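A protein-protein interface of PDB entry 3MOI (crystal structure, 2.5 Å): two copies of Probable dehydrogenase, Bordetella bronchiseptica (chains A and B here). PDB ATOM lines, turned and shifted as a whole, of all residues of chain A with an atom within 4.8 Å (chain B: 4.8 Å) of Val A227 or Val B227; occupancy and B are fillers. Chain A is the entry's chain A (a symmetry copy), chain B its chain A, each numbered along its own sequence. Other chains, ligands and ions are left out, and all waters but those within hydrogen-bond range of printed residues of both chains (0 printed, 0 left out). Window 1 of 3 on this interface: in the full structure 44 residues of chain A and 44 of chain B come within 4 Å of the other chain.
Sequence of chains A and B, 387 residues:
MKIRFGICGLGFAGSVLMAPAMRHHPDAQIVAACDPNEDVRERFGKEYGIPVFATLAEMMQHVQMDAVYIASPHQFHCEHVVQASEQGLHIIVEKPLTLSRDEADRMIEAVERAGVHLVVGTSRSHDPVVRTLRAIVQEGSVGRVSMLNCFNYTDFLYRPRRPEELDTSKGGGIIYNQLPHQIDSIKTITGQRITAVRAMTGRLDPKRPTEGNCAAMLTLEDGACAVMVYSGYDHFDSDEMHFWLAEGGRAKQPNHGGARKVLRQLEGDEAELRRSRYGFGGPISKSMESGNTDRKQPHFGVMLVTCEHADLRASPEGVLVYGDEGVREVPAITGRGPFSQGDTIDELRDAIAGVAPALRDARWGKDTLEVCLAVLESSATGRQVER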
ATOM      1  N   LEU A 148      22.837 -24.872  14.086  1.00  0.00           N
ATOM      2  CA  LEU A 148      21.717 -24.657  14.985  1.00  0.00           C
ATOM      3  C   LEU A 148      22.040 -25.196  16.353  1.00  0.00           C
ATOM      4  O   LEU A 148      22.760 -26.164  16.468  1.00  0.00           O
ATOM      5  CB  LEU A 148      20.505 -25.444  14.512  1.00  0.00           C
ATOM      6  CG  LEU A 148      19.661 -24.877  13.377  1.00  0.00           C
ATOM      7  CD1 LEU A 148      20.334 -25.288  12.080  1.00  0.00           C
ATOM      8  CD2 LEU A 148      18.311 -25.418  13.504  1.00  0.00           C
ATOM      9  N   ASN A 149      21.432 -24.628  17.386  1.00  0.00           N
ATOM     10  CA  ASN A 149      21.571 -25.168  18.740  1.00  0.00           C
ATOM     11  C   ASN A 149      20.216 -25.300  19.398  1.00  0.00           C
ATOM     12  O   ASN A 149      19.569 -24.335  19.608  1.00  0.00           O
ATOM     13  CB  ASN A 149      22.472 -24.218  19.512  1.00  0.00           C
ATOM     14  CG  ASN A 149      22.853 -24.731  20.890  1.00  0.00           C
ATOM     15  OD1 ASN A 149      22.620 -25.886  21.225  1.00  0.00           O
ATOM     16  ND2 ASN A 149      23.476 -23.865  21.692  1.00  0.00           N
ATOM     17  N   CYS A 150      19.750 -26.496  19.682  1.00  0.00           N
ATOM     18  CA  CYS A 150      18.452 -26.680  20.306  1.00  0.00           C
ATOM     19  C   CYS A 150      18.652 -27.402  21.603  1.00  0.00           C
ATOM     20  O   CYS A 150      19.309 -28.435  21.591  1.00  0.00           O
ATOM     21  CB  CYS A 150      17.547 -27.576  19.408  1.00  0.00           C
ATOM     22  SG  CYS A 150      17.487 -26.915  17.716  1.00  0.00           S
ATOM     23  N   ALA A 215      22.315 -36.314  24.120  1.00  0.00           N
ATOM     24  CA  ALA A 215      23.104 -35.277  23.504  1.00  0.00           C
ATOM     25  C   ALA A 215      23.469 -35.735  22.101  1.00  0.00           C
ATOM     26  O   ALA A 215      23.976 -36.861  21.943  1.00  0.00           O
ATOM     27  CB  ALA A 215      24.407 -34.915  24.379  1.00  0.00           C
ATOM     28  N   ALA A 216      23.212 -34.869  21.113  1.00  0.00           N
ATOM     29  CA  ALA A 216      23.473 -35.205  19.699  1.00  0.00           C
ATOM     30  C   ALA A 216      23.957 -34.065  18.859  1.00  0.00           C
ATOM     31  O   ALA A 216      23.560 -32.923  19.061  1.00  0.00           O
ATOM     32  CB  ALA A 216      22.192 -35.817  18.997  1.00  0.00           C
ATOM     33  N   MET A 217      24.785 -34.420  17.877  1.00  0.00           N
ATOM     34  CA  MET A 217      25.194 -33.539  16.846  1.00  0.00           C
ATOM     35  C   MET A 217      24.738 -34.145  15.523  1.00  0.00           C
ATOM     36  O   MET A 217      25.172 -35.273  15.112  1.00  0.00           O
ATOM     37  CB  MET A 217      26.707 -33.300  16.812  1.00  0.00           C
ATOM     38  CG  MET A 217      26.970 -31.953  16.042  1.00  0.00           C
ATOM     39  SD  MET A 217      28.587 -31.309  15.833  1.00  0.00           S
ATOM     40  CE  MET A 217      29.109 -32.170  17.186  1.00  0.00           C
ATOM     41  N   CYS A 225      25.732 -27.991  10.692  1.00  0.00           N
ATOM     42  CA  CYS A 225      25.299 -28.942  11.746  1.00  0.00           C
ATOM     43  C   CYS A 225      24.319 -28.369  12.767  1.00  0.00           C
ATOM     44  O   CYS A 225      24.275 -27.181  12.974  1.00  0.00           O
ATOM     45  CB  CYS A 225      26.490 -29.458  12.513  1.00  0.00           C
ATOM     46  SG  CYS A 225      27.733 -30.210  11.416  1.00  0.00           S
ATOM     47  N   ALA A 226      23.553 -29.248  13.398  1.00  0.00           N
ATOM     48  CA  ALA A 226      22.638 -28.921  14.463  1.00  0.00           C
ATOM     49  C   ALA A 226      23.004 -29.713  15.726  1.00  0.00           C
ATOM     50  O   ALA A 226      23.175 -30.905  15.694  1.00  0.00           O
ATOM     51  CB  ALA A 226      21.310 -29.308  14.066  1.00  0.00           C
ATOM     52  N   VAL A 227      23.144 -29.048  16.846  1.00  0.00           N
ATOM     53  CA  VAL A 227      23.290 -29.737  18.108  1.00  0.00           C
ATOM     54  C   VAL A 227      21.907 -29.849  18.712  1.00  0.00           C
ATOM     55  O   VAL A 227      21.166 -28.880  18.712  1.00  0.00           O
ATOM     56  CB  VAL A 227      24.221 -28.902  19.068  1.00  0.00           C
ATOM     57  CG1 VAL A 227      23.980 -29.230  20.561  1.00  0.00           C
ATOM     58  CG2 VAL A 227      25.666 -29.089  18.703  1.00  0.00           C
ATOM     59  N   MET A 228      21.583 -31.012  19.269  1.00  0.00           N
ATOM     60  CA  MET A 228      20.272 -31.290  19.862  1.00  0.00           C
ATOM     61  C   MET A 228      20.584 -31.922  21.218  1.00  0.00           C
ATOM     62  O   MET A 228      21.338 -32.904  21.293  1.00  0.00           O
ATOM     63  CB  MET A 228      19.510 -32.242  18.939  1.00  0.00           C
ATOM     64  CG  MET A 228      18.171 -32.785  19.373  1.00  0.00           C
ATOM     65  SD  MET A 228      17.478 -34.091  18.242  1.00  0.00           S
ATOM     66  CE  MET A 228      18.302 -33.497  16.873  1.00  0.00           C
ATOM     67  N   VAL A 229      20.057 -31.316  22.276  1.00  0.00           N
ATOM     68  CA  VAL A 229      20.217 -31.792  23.627  1.00  0.00           C
ATOM     69  C   VAL A 229      18.859 -31.832  24.305  1.00  0.00           C
ATOM     70  O   VAL A 229      18.071 -30.894  24.203  1.00  0.00           O
ATOM     71  CB  VAL A 229      21.139 -30.853  24.469  1.00  0.00           C
ATOM     72  CG1 VAL A 229      21.037 -31.210  25.975  1.00  0.00           C
ATOM     73  CG2 VAL A 229      22.583 -30.911  24.007  1.00  0.00           C
ATOM     74  N   LEU B 148      27.417 -32.998  29.457  1.00  0.00           N
ATOM     75  CA  LEU B 148      27.508 -31.574  29.731  1.00  0.00           C
ATOM     76  C   LEU B 148      27.029 -30.786  28.541  1.00  0.00           C
ATOM     77  O   LEU B 148      27.190 -31.221  27.421  1.00  0.00           O
ATOM     78  CB  LEU B 148      28.960 -31.169  29.930  1.00  0.00           C
ATOM     79  CG  LEU B 148      29.616 -31.438  31.279  1.00  0.00           C
ATOM     80  CD1 LEU B 148      30.105 -32.875  31.253  1.00  0.00           C
ATOM     81  CD2 LEU B 148      30.704 -30.480  31.451  1.00  0.00           C
ATOM     82  N   ASN B 149      26.524 -29.582  28.776  1.00  0.00           N
ATOM     83  CA  ASN B 149      26.160 -28.684  27.679  1.00  0.00           C
ATOM     84  C   ASN B 149      26.731 -27.304  27.914  1.00  0.00           C
ATOM     85  O   ASN B 149      26.376 -26.673  28.846  1.00  0.00           O
ATOM     86  CB  ASN B 149      24.642 -28.651  27.610  1.00  0.00           C
ATOM     87  CG  ASN B 149      24.106 -27.893  26.407  1.00  0.00           C
ATOM     88  OD1 ASN B 149      24.846 -27.544  25.496  1.00  0.00           O
ATOM     89  ND2 ASN B 149      22.793 -27.658  26.393  1.00  0.00           N
ATOM     90  N   CYS B 150      27.658 -26.842  27.104  1.00  0.00           N
ATOM     91  CA  CYS B 150      28.246 -25.527  27.290  1.00  0.00           C
ATOM     92  C   CYS B 150      27.993 -24.721  26.054  1.00  0.00           C
ATOM     93  O   CYS B 150      28.294 -25.213  24.973  1.00  0.00           O
ATOM     94  CB  CYS B 150      29.790 -25.650  27.459  1.00  0.00           C
ATOM     95  SG  CYS B 150      30.188 -26.848  28.767  1.00  0.00           S
ATOM     96  N   ALA B 215      30.530 -25.679  16.471  1.00  0.00           N
ATOM     97  CA  ALA B 215      29.674 -26.611  17.162  1.00  0.00           C
ATOM     98  C   ALA B 215      30.424 -27.927  17.295  1.00  0.00           C
ATOM     99  O   ALA B 215      30.942 -28.435  16.285  1.00  0.00           O
ATOM    100  CB  ALA B 215      28.259 -26.795  16.415  1.00  0.00           C
ATOM    101  N   ALA B 216      30.470 -28.457  18.524  1.00  0.00           N
ATOM    102  CA  ALA B 216      31.205 -29.707  18.803  1.00  0.00           C
ATOM    103  C   ALA B 216      30.566 -30.601  19.819  1.00  0.00           C
ATOM    104  O   ALA B 216      29.951 -30.132  20.770  1.00  0.00           O
ATOM    105  CB  ALA B 216      32.690 -29.421  19.272  1.00  0.00           C
ATOM    106  N   MET B 217      30.777 -31.901  19.616  1.00  0.00           N
ATOM    107  CA  MET B 217      30.443 -32.901  20.562  1.00  0.00           C
ATOM    108  C   MET B 217      31.734 -33.624  20.933  1.00  0.00           C
ATOM    109  O   MET B 217      32.416 -34.274  20.073  1.00  0.00           O
ATOM    110  CB  MET B 217      29.415 -33.912  20.043  1.00  0.00           C
ATOM    111  CG  MET B 217      28.736 -34.597  21.287  1.00  0.00           C
ATOM    112  SD  MET B 217      27.463 -35.788  21.104  1.00  0.00           S
ATOM    113  CE  MET B 217      27.086 -35.158  19.586  1.00  0.00           C
ATOM    114  N   CYS B 225      29.375 -37.605  27.320  1.00  0.00           N
ATOM    115  CA  CYS B 225      29.759 -36.575  26.322  1.00  0.00           C
ATOM    116  C   CYS B 225      29.474 -35.135  26.743  1.00  0.00           C
ATOM    117  O   CYS B 225      28.620 -34.892  27.560  1.00  0.00           O
ATOM    118  CB  CYS B 225      29.038 -36.809  25.019  1.00  0.00           C
ATOM    119  SG  CYS B 225      29.323 -38.488  24.376  1.00  0.00           S
ATOM    120  N   ALA B 226      30.205 -34.199  26.151  1.00  0.00           N
ATOM    121  CA  ALA B 226      30.024 -32.781  26.336  1.00  0.00           C
ATOM    122  C   ALA B 226      29.735 -32.113  24.985  1.00  0.00           C
ATOM    123  O   ALA B 226      30.435 -32.308  24.024  1.00  0.00           O
ATOM    124  CB  ALA B 226      31.244 -32.224  26.856  1.00  0.00           C
ATOM    125  N   VAL B 227      28.687 -31.332  24.900  1.00  0.00           N
ATOM    126  CA  VAL B 227      28.460 -30.514  23.730  1.00  0.00           C
ATOM    127  C   VAL B 227      29.059 -29.155  24.019  1.00  0.00           C
ATOM    128  O   VAL B 227      28.855 -28.620  25.095  1.00  0.00           O
ATOM    129  CB  VAL B 227      26.911 -30.366  23.474  1.00  0.00           C
ATOM    130  CG1 VAL B 227      26.565 -29.102  22.650  1.00  0.00           C
ATOM    131  CG2 VAL B 227      26.360 -31.601  22.821  1.00  0.00           C
ATOM    132  N   MET B 228      29.753 -28.580  23.041  1.00  0.00           N
ATOM    133  CA  MET B 228      30.426 -27.285  23.176  1.00  0.00           C
ATOM    134  C   MET B 228      30.019 -26.503  21.927  1.00  0.00           C
ATOM    135  O   MET B 228      30.189 -26.992  20.799  1.00  0.00           O
ATOM    136  CB  MET B 228      31.934 -27.522  23.247  1.00  0.00           C
ATOM    137  CG  MET B 228      32.873 -26.341  23.270  1.00  0.00           C
ATOM    138  SD  MET B 228      34.673 -26.797  23.140  1.00  0.00           S
ATOM    139  CE  MET B 228      34.443 -28.339  23.831  1.00  0.00           C
ATOM    140  N   VAL B 229      29.430 -25.332  22.141  1.00  0.00           N
ATOM    141  CA  VAL B 229      29.013 -24.447  21.083  1.00  0.00           C
ATOM    142  C   VAL B 229      29.515 -23.045  21.380  1.00  0.00           C
ATOM    143  O   VAL B 229      29.408 -22.557  22.503  1.00  0.00           O
ATOM    144  CB  VAL B 229      27.457 -24.377  20.964  1.00  0.00           C
ATOM    145  CG1 VAL B 229      27.041 -23.196  20.047  1.00  0.00           C
ATOM    146  CG2 VAL B 229      26.866 -25.677  20.453  1.00  0.00           C
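SD of Met A217 lies close to O of Ala B215. O of Ala A215 lies close to SD of Met B217.
The backbone carbonyl oxygen (O) of Leu A148 sits at hydrogen-bond distance from the backbone NH (N) of Val A227 (2.9 Å). The backbone NH of Cys B150 is in hydrogen-bond range of the backbone carbonyl oxygen of Val B227, 2.9 Å away. The backbone NH (N) of Val A229 sits at hydrogen-bond distance from the backbone carbonyl oxygen (O) of Cys A150 (3.1 Å). The backbone carbonyl oxygen of Met B228 is in hydrogen-bond range of the backbone NH of Ala B216 (2.7 Å). N of Val B229 is in hydrogen-bond range of O of Cys B150 (3.1 Å). N of Cys A150 is in hydrogen-bond range of O of Val A227, at 2.9 Å.
Among the printed residues, pairs that only touch across the chains: Met A217 with Met B217 (3.0 Å), Val A227 with Val B227 (3.3 Å), Ala A216 with Met B217 (3.4 Å), Met A217 with Ala B216 (3.4 Å), Asn A149 with Val B229 (3.98 Å) and Val A229 with Asn B149 (3.98 Å).
Printed residues of chain B within 4 Å of Asn A149: Val B229. Printed residues of chain B within 4 Å of Ala A216: Met B217 (3.4 Å). Ala A226 touches none of the printed residues of chain B. Of the printed residues of chain B, Val A227 touches Val B227. Of the printed residues of chain A, Ala B215 touches Met A217 (3.7 Å). Of the printed residues of chain A, Val B227 touches Val A227. Met B228 touches none of the printed residues of chain A. The nearest printed residue of chain B that does not touch Val A227 is Val B229 (4.02 Å).
Of the 11 printed residues of chain B, 6 touch a printed residue of chain A.
Asn A149 touches Val B229, and with the chains exchanged Val A229 touches Asn B149. Ala A215 touches Met B217, and with the chains exchanged Met A217 touches Ala B215. Met A217 touches its own counterpart, Met B217. Val A227 touches its own counterpart, Val B227. 11 positions are printed for both chains.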
